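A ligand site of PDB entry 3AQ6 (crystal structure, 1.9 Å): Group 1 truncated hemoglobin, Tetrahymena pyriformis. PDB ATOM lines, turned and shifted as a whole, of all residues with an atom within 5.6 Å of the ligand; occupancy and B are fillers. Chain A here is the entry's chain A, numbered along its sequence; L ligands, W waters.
Residues that only touch the ligand: Phe 37 (3.3 Å), Phe 38 (3.2 Å), Gln 46 (3.4 Å), Gln 49 (3.7 Å), Gln 50 (3.3 Å), Phe 53 (3.6 Å), Tyr 64 (3.6 Å), Gly 66 (3.3 Å), Met 69 (3.5 Å), Ala 72 (3.7 Å), Met 76 (3.4 Å), Leu 78 (3.8 Å), His 82 (3.6 Å), Phe 83 (3.4 Å), Ile 86 (3.3 Å), Ile 111 (3.6 Å), Thr 114 (3.5 Å) and Met 118 (3.3 Å).
ND1 of His 73 is in hydrogen-bond range of O of Met 69, 2.7 Å away.
O of Lys 67 sits at hydrogen-bond distance from OH of Tyr 64 (2.6 Å).
The side-chain hydroxyl of Tyr 25 lies within hydrogen-bond range of the side-chain amide nitrogen of Gln 50 (3.0 Å).
NE2 of Gln 46 lies within hydrogen-bond range of OH of Tyr 25.
OG1 of Thr 114 lies within hydrogen-bond range of O of Ile 111.
Water W2 bridges the side-chain hydroxyl of Tyr 25 (3.1 Å) and the side-chain amide nitrogen of Gln 50 (3.3 Å).
Water W3 lies within hydrogen-bond range of O of Ala 72 (2.7 Å) and O1 of the ligand (3.3 Å).
NE2 of His 73 is bound to FE1 of the ligand.
The backbone NH (N) of Lys 67 sits at hydrogen-bond distance from an oxygen (O3) of the ligand.
OG1 of Thr 41 is in hydrogen-bond range of O2 of the ligand (3.0 Å).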
ATOM      1  N   TYR A  25     -28.180   7.215 -13.489  1.00  0.00           N
ATOM      2  CA  TYR A  25     -27.087   6.277 -13.057  1.00  0.00           C
ATOM      3  C   TYR A  25     -27.100   4.928 -13.760  1.00  0.00           C
ATOM      4  O   TYR A  25     -26.022   4.359 -14.042  1.00  0.00           O
ATOM      5  CB  TYR A  25     -27.012   6.163 -11.487  1.00  0.00           C
ATOM      6  CG  TYR A  25     -26.275   7.448 -10.917  1.00  0.00           C
ATOM      7  CD1 TYR A  25     -26.948   8.325 -10.046  1.00  0.00           C
ATOM      8  CD2 TYR A  25     -24.971   7.805 -11.335  1.00  0.00           C
ATOM      9  CE1 TYR A  25     -26.360   9.495  -9.544  1.00  0.00           C
ATOM     10  CE2 TYR A  25     -24.354   9.018 -10.850  1.00  0.00           C
ATOM     11  CZ  TYR A  25     -25.036   9.844  -9.957  1.00  0.00           C
ATOM     12  OH  TYR A  25     -24.404  10.972  -9.499  1.00  0.00           O
ATOM     13  N   VAL A  34     -17.153   6.338 -18.315  1.00  0.00           N
ATOM     14  CA  VAL A  34     -17.309   6.857 -16.933  1.00  0.00           C
ATOM     15  C   VAL A  34     -17.669   5.833 -15.819  1.00  0.00           C
ATOM     16  O   VAL A  34     -17.566   6.167 -14.623  1.00  0.00           O
ATOM     17  CB  VAL A  34     -18.319   8.089 -16.856  1.00  0.00           C
ATOM     18  CG1 VAL A  34     -17.745   9.294 -17.654  1.00  0.00           C
ATOM     19  CG2 VAL A  34     -19.637   7.780 -17.405  1.00  0.00           C
ATOM     20  N   PHE A  37     -15.549   5.157 -12.553  1.00  0.00           N
ATOM     21  CA  PHE A  37     -15.326   6.173 -11.501  1.00  0.00           C
ATOM     22  C   PHE A  37     -16.178   5.898 -10.247  1.00  0.00           C
ATOM     23  O   PHE A  37     -15.801   6.295  -9.128  1.00  0.00           O
ATOM     24  CB  PHE A  37     -15.594   7.563 -12.007  1.00  0.00           C
ATOM     25  CG  PHE A  37     -14.523   8.013 -12.941  1.00  0.00           C
ATOM     26  CD1 PHE A  37     -14.733   7.966 -14.304  1.00  0.00           C
ATOM     27  CD2 PHE A  37     -13.329   8.448 -12.435  1.00  0.00           C
ATOM     28  CE1 PHE A  37     -13.683   8.342 -15.185  1.00  0.00           C
ATOM     29  CE2 PHE A  37     -12.305   8.819 -13.282  1.00  0.00           C
ATOM     30  CZ  PHE A  37     -12.497   8.771 -14.677  1.00  0.00           C
ATOM     31  N   PHE A  38     -17.311   5.263 -10.473  1.00  0.00           N
ATOM     32  CA  PHE A  38     -18.242   4.906  -9.418  1.00  0.00           C
ATOM     33  C   PHE A  38     -18.042   3.554  -8.780  1.00  0.00           C
ATOM     34  O   PHE A  38     -18.928   3.071  -7.995  1.00  0.00           O
ATOM     35  CB  PHE A  38     -19.712   4.996  -9.946  1.00  0.00           C
ATOM     36  CG  PHE A  38     -20.056   6.380 -10.421  1.00  0.00           C
ATOM     37  CD1 PHE A  38     -19.711   6.802 -11.740  1.00  0.00           C
ATOM     38  CD2 PHE A  38     -20.511   7.332  -9.515  1.00  0.00           C
ATOM     39  CE1 PHE A  38     -19.925   8.131 -12.150  1.00  0.00           C
ATOM     40  CE2 PHE A  38     -20.708   8.689  -9.925  1.00  0.00           C
ATOM     41  CZ  PHE A  38     -20.437   9.098 -11.231  1.00  0.00           C
ATOM     42  N   ASN A  40     -16.331   2.276  -6.346  1.00  0.00           N
ATOM     43  CA  ASN A  40     -16.416   2.231  -4.873  1.00  0.00           C
ATOM     44  C   ASN A  40     -17.440   3.205  -4.231  1.00  0.00           C
ATOM     45  O   ASN A  40     -17.453   3.355  -3.016  1.00  0.00           O
ATOM     46  CB  ASN A  40     -15.040   2.484  -4.252  1.00  0.00           C
ATOM     47  CG  ASN A  40     -14.037   1.424  -4.670  1.00  0.00           C
ATOM     48  OD1 ASN A  40     -14.297   0.242  -4.542  1.00  0.00           O
ATOM     49  ND2 ASN A  40     -12.921   1.850  -5.195  1.00  0.00           N
ATOM     50  N   THR A  41     -18.325   3.769  -5.032  1.00  0.00           N
ATOM     51  CA  THR A  41     -19.367   4.676  -4.549  1.00  0.00           C
ATOM     52  C   THR A  41     -20.613   3.948  -3.995  1.00  0.00           C
ATOM     53  O   THR A  41     -21.101   2.917  -4.553  1.00  0.00           O
ATOM     54  CB  THR A  41     -19.701   5.716  -5.649  1.00  0.00           C
ATOM     55  OG1 THR A  41     -18.537   6.455  -5.905  1.00  0.00           O
ATOM     56  CG2 THR A  41     -20.761   6.749  -5.135  1.00  0.00           C
ATOM     57  N   ASP A  42     -21.042   4.378  -2.810  1.00  0.00           N
ATOM     58  CA  ASP A  42     -22.347   3.946  -2.261  1.00  0.00           C
ATOM     59  C   ASP A  42     -23.414   4.613  -3.196  1.00  0.00           C
ATOM     60  O   ASP A  42     -23.627   5.869  -3.112  1.00  0.00           O
ATOM     61  CB  ASP A  42     -22.482   4.456  -0.819  1.00  0.00           C
ATOM     62  CG  ASP A  42     -23.838   4.110  -0.179  1.00  0.00           C
ATOM     63  OD1 ASP A  42     -24.897   3.907  -0.890  1.00  0.00           O
ATOM     64  OD2 ASP A  42     -23.830   4.036   1.083  1.00  0.00           O
ATOM     65  N   HIS A  45     -26.406   6.531  -1.433  1.00  0.00           N
ATOM     66  CA  HIS A  45     -25.982   7.866  -1.026  1.00  0.00           C
ATOM     67  C   HIS A  45     -25.825   8.776  -2.223  1.00  0.00           C
ATOM     68  O   HIS A  45     -26.293   9.930  -2.198  1.00  0.00           O
ATOM     69  CB  HIS A  45     -24.702   7.848  -0.203  1.00  0.00           C
ATOM     70  CG  HIS A  45     -24.387   9.163   0.459  1.00  0.00           C
ATOM     71  ND1 HIS A  45     -23.313   9.930   0.074  1.00  0.00           N
ATOM     72  CD2 HIS A  45     -25.009   9.851   1.451  1.00  0.00           C
ATOM     73  CE1 HIS A  45     -23.261  11.026   0.817  1.00  0.00           C
ATOM     74  NE2 HIS A  45     -24.286  11.020   1.643  1.00  0.00           N
ATOM     75  N   GLN A  46     -25.104   8.338  -3.266  1.00  0.00           N
ATOM     76  CA  GLN A  46     -24.822   9.218  -4.398  1.00  0.00           C
ATOM     77  C   GLN A  46     -26.160   9.636  -5.075  1.00  0.00           C
ATOM     78  O   GLN A  46     -26.341  10.755  -5.542  1.00  0.00           O
ATOM     79  CB  GLN A  46     -23.950   8.435  -5.408  1.00  0.00           C
ATOM     80  CG  GLN A  46     -23.633   9.159  -6.688  1.00  0.00           C
ATOM     81  CD  GLN A  46     -22.828  10.418  -6.366  1.00  0.00           C
ATOM     82  OE1 GLN A  46     -22.210  10.486  -5.304  1.00  0.00           O
ATOM     83  NE2 GLN A  46     -22.907  11.435  -7.209  1.00  0.00           N
ATOM     84  N   GLN A  49     -27.682  12.419  -2.991  1.00  0.00           N
ATOM     85  CA  GLN A  49     -26.948  13.664  -3.138  1.00  0.00           C
ATOM     86  C   GLN A  49     -27.208  14.284  -4.474  1.00  0.00           C
ATOM     87  O   GLN A  49     -27.365  15.530  -4.590  1.00  0.00           O
ATOM     88  CB  GLN A  49     -25.412  13.447  -3.000  1.00  0.00           C
ATOM     89  CG  GLN A  49     -25.015  13.085  -1.541  1.00  0.00           C
ATOM     90  CD  GLN A  49     -25.407  14.198  -0.527  1.00  0.00           C
ATOM     91  OE1 GLN A  49     -24.811  15.231  -0.479  1.00  0.00           O
ATOM     92  NE2 GLN A  49     -26.313  13.945   0.275  1.00  0.00           N
ATOM     93  N   GLN A  50     -27.232  13.467  -5.515  1.00  0.00           N
ATOM     94  CA  GLN A  50     -27.308  14.052  -6.867  1.00  0.00           C
ATOM     95  C   GLN A  50     -28.769  14.498  -7.059  1.00  0.00           C
ATOM     96  O   GLN A  50     -29.028  15.457  -7.690  1.00  0.00           O
ATOM     97  CB  GLN A  50     -26.948  12.978  -7.944  1.00  0.00           C
ATOM     98  CG  GLN A  50     -27.065  13.475  -9.402  1.00  0.00           C
ATOM     99  CD  GLN A  50     -25.893  14.432  -9.712  1.00  0.00           C
ATOM    100  OE1 GLN A  50     -26.021  15.650  -9.540  1.00  0.00           O
ATOM    101  NE2 GLN A  50     -24.747  13.880 -10.073  1.00  0.00           N
ATOM    102  N   PHE A  53     -28.858  17.750  -5.412  1.00  0.00           N
ATOM    103  CA  PHE A  53     -28.102  18.744  -6.127  1.00  0.00           C
ATOM    104  C   PHE A  53     -28.799  19.250  -7.384  1.00  0.00           C
ATOM    105  O   PHE A  53     -28.949  20.476  -7.579  1.00  0.00           O
ATOM    106  CB  PHE A  53     -26.685  18.196  -6.539  1.00  0.00           C
ATOM    107  CG  PHE A  53     -25.763  19.297  -7.093  1.00  0.00           C
ATOM    108  CD1 PHE A  53     -25.263  20.268  -6.256  1.00  0.00           C
ATOM    109  CD2 PHE A  53     -25.458  19.370  -8.456  1.00  0.00           C
ATOM    110  CE1 PHE A  53     -24.342  21.310  -6.729  1.00  0.00           C
ATOM    111  CE2 PHE A  53     -24.575  20.393  -8.934  1.00  0.00           C
ATOM    112  CZ  PHE A  53     -24.041  21.354  -8.090  1.00  0.00           C
ATOM    113  N   LEU A  54     -29.248  18.338  -8.245  1.00  0.00           N
ATOM    114  CA  LEU A  54     -29.964  18.812  -9.423  1.00  0.00           C
ATOM    115  C   LEU A  54     -31.287  19.455  -9.059  1.00  0.00           C
ATOM    116  O   LEU A  54     -31.753  20.347  -9.760  1.00  0.00           O
ATOM    117  CB  LEU A  54     -30.306  17.637 -10.346  1.00  0.00           C
ATOM    118  CG  LEU A  54     -29.036  17.070 -11.055  1.00  0.00           C
ATOM    119  CD1 LEU A  54     -29.441  15.701 -11.731  1.00  0.00           C
ATOM    120  CD2 LEU A  54     -28.262  18.021 -11.968  1.00  0.00           C
ATOM    121  N   LEU A  57     -30.263  22.866  -8.246  1.00  0.00           N
ATOM    122  CA  LEU A  57     -29.717  23.604  -9.375  1.00  0.00           C
ATOM    123  C   LEU A  57     -30.803  24.097 -10.377  1.00  0.00           C
ATOM    124  O   LEU A  57     -30.672  25.191 -10.967  1.00  0.00           O
ATOM    125  CB  LEU A  57     -28.768  22.674 -10.140  1.00  0.00           C
ATOM    126  CG  LEU A  57     -27.674  23.440 -10.896  1.00  0.00           C
ATOM    127  CD1 LEU A  57     -26.631  24.264 -10.002  1.00  0.00           C
ATOM    128  CD2 LEU A  57     -26.969  22.324 -11.713  1.00  0.00           C
ATOM    129  N   TYR A  64     -29.699  20.795  -0.671  1.00  0.00           N
ATOM    130  CA  TYR A  64     -28.419  20.194  -0.991  1.00  0.00           C
ATOM    131  C   TYR A  64     -27.426  20.543   0.067  1.00  0.00           C
ATOM    132  O   TYR A  64     -27.055  21.721   0.223  1.00  0.00           O
ATOM    133  CB  TYR A  64     -27.880  20.697  -2.356  1.00  0.00           C
ATOM    134  CG  TYR A  64     -26.533  20.075  -2.662  1.00  0.00           C
ATOM    135  CD1 TYR A  64     -26.425  18.691  -2.827  1.00  0.00           C
ATOM    136  CD2 TYR A  64     -25.358  20.837  -2.753  1.00  0.00           C
ATOM    137  CE1 TYR A  64     -25.179  18.058  -3.070  1.00  0.00           C
ATOM    138  CE2 TYR A  64     -24.128  20.239  -3.012  1.00  0.00           C
ATOM    139  CZ  TYR A  64     -24.058  18.815  -3.194  1.00  0.00           C
ATOM    140  OH  TYR A  64     -22.839  18.181  -3.449  1.00  0.00           O
ATOM    141  N   GLY A  66     -24.282  18.662   0.304  1.00  0.00           N
ATOM    142  CA  GLY A  66     -22.985  18.047   0.068  1.00  0.00           C
ATOM    143  C   GLY A  66     -21.854  19.012  -0.379  1.00  0.00           C
ATOM    144  O   GLY A  66     -21.927  20.233  -0.183  1.00  0.00           O
ATOM    145  N   LYS A  67     -20.785  18.466  -0.934  1.00  0.00           N
ATOM    146  CA  LYS A  67     -19.653  19.212  -1.295  1.00  0.00           C
ATOM    147  C   LYS A  67     -19.920  20.072  -2.529  1.00  0.00           C
ATOM    148  O   LYS A  67     -20.798  19.790  -3.336  1.00  0.00           O
ATOM    149  CB  LYS A  67     -18.508  18.261  -1.588  1.00  0.00           C
ATOM    150  CG  LYS A  67     -17.978  17.579  -0.295  1.00  0.00           C
ATOM    151  CD  LYS A  67     -17.236  16.312  -0.692  1.00  0.00           C
ATOM    152  CE  LYS A  67     -16.877  15.473   0.572  1.00  0.00           C
ATOM    153  NZ  LYS A  67     -16.481  14.125   0.113  1.00  0.00           N
ATOM    154  N   MET A  69     -18.551  21.405  -6.318  1.00  0.00           N
ATOM    155  CA  MET A  69     -18.189  20.559  -7.443  1.00  0.00           C
ATOM    156  C   MET A  69     -16.702  20.358  -7.555  1.00  0.00           C
ATOM    157  O   MET A  69     -16.252  19.340  -8.169  1.00  0.00           O
ATOM    158  CB  MET A  69     -18.828  21.093  -8.741  1.00  0.00           C
ATOM    159  CG  MET A  69     -20.401  20.892  -8.762  1.00  0.00           C
ATOM    160  SD  MET A  69     -20.910  19.165  -8.615  1.00  0.00           S
ATOM    161  CE  MET A  69     -21.331  19.075  -6.868  1.00  0.00           C
ATOM    162  N   ALA A  72     -16.095  17.768  -4.495  1.00  0.00           N
ATOM    163  CA  ALA A  72     -16.684  16.465  -4.872  1.00  0.00           C
ATOM    164  C   ALA A  72     -15.761  15.634  -5.814  1.00  0.00           C
ATOM    165  O   ALA A  72     -15.763  14.430  -5.715  1.00  0.00           O
ATOM    166  CB  ALA A  72     -17.961  16.633  -5.510  1.00  0.00           C
ATOM    167  N   HIS A  73     -15.055  16.290  -6.732  1.00  0.00           N
ATOM    168  CA  HIS A  73     -14.262  15.559  -7.759  1.00  0.00           C
ATOM    169  C   HIS A  73     -12.776  15.786  -7.570  1.00  0.00           C
ATOM    170  O   HIS A  73     -11.987  15.594  -8.542  1.00  0.00           O
ATOM    171  CB  HIS A  73     -14.744  16.042  -9.168  1.00  0.00           C
ATOM    172  CG  HIS A  73     -16.224  15.908  -9.322  1.00  0.00           C
ATOM    173  ND1 HIS A  73     -17.118  16.934  -9.014  1.00  0.00           N
ATOM    174  CD2 HIS A  73     -16.984  14.806  -9.570  1.00  0.00           C
ATOM    175  CE1 HIS A  73     -18.346  16.493  -9.224  1.00  0.00           C
ATOM    176  NE2 HIS A  73     -18.284  15.221  -9.562  1.00  0.00           N
ATOM    177  N   MET A  76      -9.665  13.471  -8.874  1.00  0.00           N
ATOM    178  CA  MET A  76     -10.049  12.603 -10.003  1.00  0.00           C
ATOM    179  C   MET A  76      -9.390  13.000 -11.334  1.00  0.00           C
ATOM    180  O   MET A  76      -9.239  12.166 -12.225  1.00  0.00           O
ATOM    181  CB  MET A  76     -11.585  12.495 -10.205  1.00  0.00           C
ATOM    182  CG  MET A  76     -12.283  11.858  -8.955  1.00  0.00           C
ATOM    183  SD  MET A  76     -14.011  12.013  -9.287  1.00  0.00           S
ATOM    184  CE  MET A  76     -14.852  11.466  -7.757  1.00  0.00           C
ATOM    185  N   LEU A  78     -10.446  14.803 -13.719  1.00  0.00           N
ATOM    186  CA  LEU A  78     -11.409  14.509 -14.746  1.00  0.00           C
ATOM    187  C   LEU A  78     -11.147  15.314 -16.021  1.00  0.00           C
ATOM    188  O   LEU A  78     -10.616  16.426 -15.958  1.00  0.00           O
ATOM    189  CB  LEU A  78     -12.780  14.965 -14.257  1.00  0.00           C
ATOM    190  CG  LEU A  78     -13.710  13.968 -13.596  1.00  0.00           C
ATOM    191  CD1 LEU A  78     -13.276  12.558 -13.433  1.00  0.00           C
ATOM    192  CD2 LEU A  78     -14.606  14.547 -12.507  1.00  0.00           C
ATOM    193  N   GLN A  79     -11.444  14.662 -17.142  1.00  0.00           N
ATOM    194  CA  GLN A  79     -11.162  15.201 -18.484  1.00  0.00           C
ATOM    195  C   GLN A  79     -12.464  15.596 -19.181  1.00  0.00           C
ATOM    196  O   GLN A  79     -13.557  15.074 -18.885  1.00  0.00           O
ATOM    197  CB  GLN A  79     -10.491  14.098 -19.298  1.00  0.00           C
ATOM    198  CG  GLN A  79      -9.226  13.563 -18.596  1.00  0.00           C
ATOM    199  CD  GLN A  79      -8.157  14.672 -18.541  1.00  0.00           C
ATOM    200  OE1 GLN A  79      -7.789  15.273 -19.565  1.00  0.00           O
ATOM    201  NE2 GLN A  79      -7.656  14.918 -17.346  1.00  0.00           N
ATOM    202  N   HIS A  82     -15.064  13.046 -20.027  1.00  0.00           N
ATOM    203  CA  HIS A  82     -15.903  12.482 -18.984  1.00  0.00           C
ATOM    204  C   HIS A  82     -17.115  13.374 -18.778  1.00  0.00           C
ATOM    205  O   HIS A  82     -18.190  12.859 -18.583  1.00  0.00           O
ATOM    206  CB  HIS A  82     -15.132  12.371 -17.668  1.00  0.00           C
ATOM    207  CG  HIS A  82     -13.843  11.569 -17.766  1.00  0.00           C
ATOM    208  ND1 HIS A  82     -13.800  10.243 -18.180  1.00  0.00           N
ATOM    209  CD2 HIS A  82     -12.577  11.909 -17.487  1.00  0.00           C
ATOM    210  CE1 HIS A  82     -12.541   9.812 -18.150  1.00  0.00           C
ATOM    211  NE2 HIS A  82     -11.793  10.779 -17.679  1.00  0.00           N
ATOM    212  N   PHE A  83     -16.914  14.686 -18.770  1.00  0.00           N
ATOM    213  CA  PHE A  83     -18.031  15.608 -18.550  1.00  0.00           C
ATOM    214  C   PHE A  83     -19.054  15.477 -19.708  1.00  0.00           C
ATOM    215  O   PHE A  83     -20.269  15.435 -19.447  1.00  0.00           O
ATOM    216  CB  PHE A  83     -17.506  17.098 -18.447  1.00  0.00           C
ATOM    217  CG  PHE A  83     -18.593  18.051 -18.020  1.00  0.00           C
ATOM    218  CD1 PHE A  83     -18.746  18.358 -16.675  1.00  0.00           C
ATOM    219  CD2 PHE A  83     -19.454  18.640 -18.951  1.00  0.00           C
ATOM    220  CE1 PHE A  83     -19.766  19.191 -16.212  1.00  0.00           C
ATOM    221  CE2 PHE A  83     -20.476  19.560 -18.505  1.00  0.00           C
ATOM    222  CZ  PHE A  83     -20.658  19.783 -17.113  1.00  0.00           C
ATOM    223  N   ILE A  86     -21.193  12.515 -19.079  1.00  0.00           N
ATOM    224  CA  ILE A  86     -22.219  12.688 -18.059  1.00  0.00           C
ATOM    225  C   ILE A  86     -23.430  13.462 -18.623  1.00  0.00           C
ATOM    226  O   ILE A  86     -24.609  13.044 -18.423  1.00  0.00           O
ATOM    227  CB  ILE A  86     -21.609  13.361 -16.774  1.00  0.00           C
ATOM    228  CG1 ILE A  86     -20.537  12.433 -16.149  1.00  0.00           C
ATOM    229  CG2 ILE A  86     -22.771  13.750 -15.737  1.00  0.00           C
ATOM    230  CD1 ILE A  86     -21.104  11.001 -15.513  1.00  0.00           C
ATOM    231  N   ILE A  87     -23.151  14.550 -19.333  1.00  0.00           N
ATOM    232  CA  ILE A  87     -24.214  15.439 -19.884  1.00  0.00           C
ATOM    233  C   ILE A  87     -25.007  14.699 -20.887  1.00  0.00           C
ATOM    234  O   ILE A  87     -26.303  14.724 -20.859  1.00  0.00           O
ATOM    235  CB  ILE A  87     -23.624  16.576 -20.761  1.00  0.00           C
ATOM    236  CG1 ILE A  87     -22.830  17.557 -19.920  1.00  0.00           C
ATOM    237  CG2 ILE A  87     -24.829  17.288 -21.572  1.00  0.00           C
ATOM    238  CD1 ILE A  87     -23.914  18.263 -18.878  1.00  0.00           C
ATOM    239  N   ILE A 111     -26.367  23.258 -16.140  1.00  0.00           N
ATOM    240  CA  ILE A 111     -25.358  22.268 -15.645  1.00  0.00           C
ATOM    241  C   ILE A 111     -24.017  22.499 -16.267  1.00  0.00           C
ATOM    242  O   ILE A 111     -23.002  22.295 -15.629  1.00  0.00           O
ATOM    243  CB  ILE A 111     -25.822  20.839 -15.925  1.00  0.00           C
ATOM    244  CG1 ILE A 111     -27.098  20.596 -15.129  1.00  0.00           C
ATOM    245  CG2 ILE A 111     -24.711  19.752 -15.545  1.00  0.00           C
ATOM    246  CD1 ILE A 111     -27.982  19.375 -15.605  1.00  0.00           C
ATOM    247  N   THR A 114     -20.973  24.154 -14.522  1.00  0.00           N
ATOM    248  CA  THR A 114     -20.141  23.431 -13.532  1.00  0.00           C
ATOM    249  C   THR A 114     -18.875  22.822 -14.124  1.00  0.00           C
ATOM    250  O   THR A 114     -18.017  22.323 -13.397  1.00  0.00           O
ATOM    251  CB  THR A 114     -20.882  22.307 -12.824  1.00  0.00           C
ATOM    252  OG1 THR A 114     -21.305  21.250 -13.739  1.00  0.00           O
ATOM    253  CG2 THR A 114     -22.194  22.849 -12.151  1.00  0.00           C
ATOM    254  N   MET A 118     -15.155  21.219 -12.055  1.00  0.00           N
ATOM    255  CA  MET A 118     -14.774  19.833 -11.785  1.00  0.00           C
ATOM    256  C   MET A 118     -13.698  19.192 -12.626  1.00  0.00           C
ATOM    257  O   MET A 118     -13.151  18.128 -12.237  1.00  0.00           O
ATOM    258  CB  MET A 118     -16.003  18.998 -11.862  1.00  0.00           C
ATOM    259  CG  MET A 118     -16.623  18.854 -13.241  1.00  0.00           C
ATOM    260  SD  MET A 118     -17.973  17.736 -12.904  1.00  0.00           S
ATOM    261  CE  MET A 118     -19.125  18.745 -11.979  1.00  0.00           C
ATOM    262  N   LEU A 119     -13.301  19.824 -13.750  1.00  0.00           N
ATOM    263  CA  LEU A 119     -12.290  19.216 -14.611  1.00  0.00           C
ATOM    264  C   LEU A 119     -10.899  19.431 -14.037  1.00  0.00           C
ATOM    265  O   LEU A 119     -10.577  20.534 -13.588  1.00  0.00           O
ATOM    266  CB  LEU A 119     -12.296  19.801 -16.024  1.00  0.00           C
ATOM    267  CG  LEU A 119     -13.607  19.406 -16.786  1.00  0.00           C
ATOM    268  CD1 LEU A 119     -13.346  19.849 -18.283  1.00  0.00           C
ATOM    269  CD2 LEU A 119     -13.930  17.979 -16.652  1.00  0.00           C
HETATM  270  C1  LIG L   1     -19.746  13.035  -6.495  1.00  0.00           C
HETATM  271  C2  LIG L   1     -18.071  11.142 -10.646  1.00  0.00           C
HETATM  272  C3  LIG L   1     -19.675  14.961 -13.044  1.00  0.00           C
HETATM  273  C4  LIG L   1     -22.380  16.012  -9.285  1.00  0.00           C
HETATM  274  C5  LIG L   1     -19.149  12.221  -7.444  1.00  0.00           C
HETATM  275  C6  LIG L   1     -18.448  10.978  -7.140  1.00  0.00           C
HETATM  276  C7  LIG L   1     -18.016  10.490  -8.278  1.00  0.00           C
HETATM  277  C8  LIG L   1     -18.400  11.388  -9.328  1.00  0.00           C
HETATM  278  C9  LIG L   1     -17.238   9.148  -8.496  1.00  0.00           C
HETATM  279  C10 LIG L   1     -18.368  10.253  -5.770  1.00  0.00           C
HETATM  280  C11 LIG L   1     -17.088  10.522  -5.041  1.00  0.00           C
HETATM  281  C12 LIG L   1     -17.108   9.558  -3.844  1.00  0.00           C
HETATM  282  O1  LIG L   1     -16.167   9.898  -3.026  1.00  0.00           O
HETATM  283  O2  LIG L   1     -17.920   8.502  -3.775  1.00  0.00           O
HETATM  284  C13 LIG L   1     -18.308  12.092 -11.611  1.00  0.00           C
HETATM  285  C14 LIG L   1     -17.729  12.017 -12.946  1.00  0.00           C
HETATM  286  C15 LIG L   1     -18.111  13.095 -13.582  1.00  0.00           C
HETATM  287  C16 LIG L   1     -18.960  13.849 -12.667  1.00  0.00           C
HETATM  288  C17 LIG L   1     -16.771  10.961 -13.532  1.00  0.00           C
HETATM  289  C18 LIG L   1     -17.622  13.418 -15.056  1.00  0.00           C
HETATM  290  C19 LIG L   1     -17.376  14.685 -15.299  1.00  0.00           C
HETATM  291  C20 LIG L   1     -20.650  15.491 -12.257  1.00  0.00           C
HETATM  292  C21 LIG L   1     -21.637  16.473 -12.692  1.00  0.00           C
HETATM  293  C22 LIG L   1     -22.360  16.778 -11.633  1.00  0.00           C
HETATM  294  C23 LIG L   1     -21.874  15.995 -10.551  1.00  0.00           C
HETATM  295  C24 LIG L   1     -21.731  17.038 -14.167  1.00  0.00           C
HETATM  296  C25 LIG L   1     -23.614  17.732 -11.568  1.00  0.00           C
HETATM  297  C26 LIG L   1     -23.487  18.909 -12.239  1.00  0.00           C
HETATM  298  C27 LIG L   1     -21.882  15.277  -8.268  1.00  0.00           C
HETATM  299  C28 LIG L   1     -22.418  15.443  -6.960  1.00  0.00           C
HETATM  300  C29 LIG L   1     -21.582  14.558  -6.107  1.00  0.00           C
HETATM  301  C30 LIG L   1     -20.678  13.931  -6.998  1.00  0.00           C
HETATM  302  C31 LIG L   1     -23.637  16.256  -6.402  1.00  0.00           C
HETATM  303  C32 LIG L   1     -21.731  14.302  -4.587  1.00  0.00           C
HETATM  304  C33 LIG L   1     -20.885  15.185  -3.666  1.00  0.00           C
HETATM  305  C34 LIG L   1     -21.156  14.794  -2.214  1.00  0.00           C
HETATM  306  O3  LIG L   1     -21.086  15.665  -1.282  1.00  0.00           O
HETATM  307  O4  LIG L   1     -21.331  13.558  -1.947  1.00  0.00           O
HETATM  308  N1  LIG L   1     -19.079  12.455  -8.794  1.00  0.00           N
HETATM  309  N2  LIG L   1     -19.125  13.228 -11.435  1.00  0.00           N
HETATM  310  N3  LIG L   1     -20.850  15.188 -10.971  1.00  0.00           N
HETATM  311  N4  LIG L   1     -20.802  14.386  -8.306  1.00  0.00           N
HETATM  312 FE1  LIG L   1     -19.947  13.826  -9.900  1.00  0.00          FE
HETATM  313  O   HOH W   1     -21.000  15.065   1.306  1.00  0.00           O
HETATM  314  O   HOH W   2     -21.822  12.401 -10.424  1.00  0.00           O
HETATM  315  O   HOH W   3     -16.609  13.182  -3.434  1.00  0.00           O
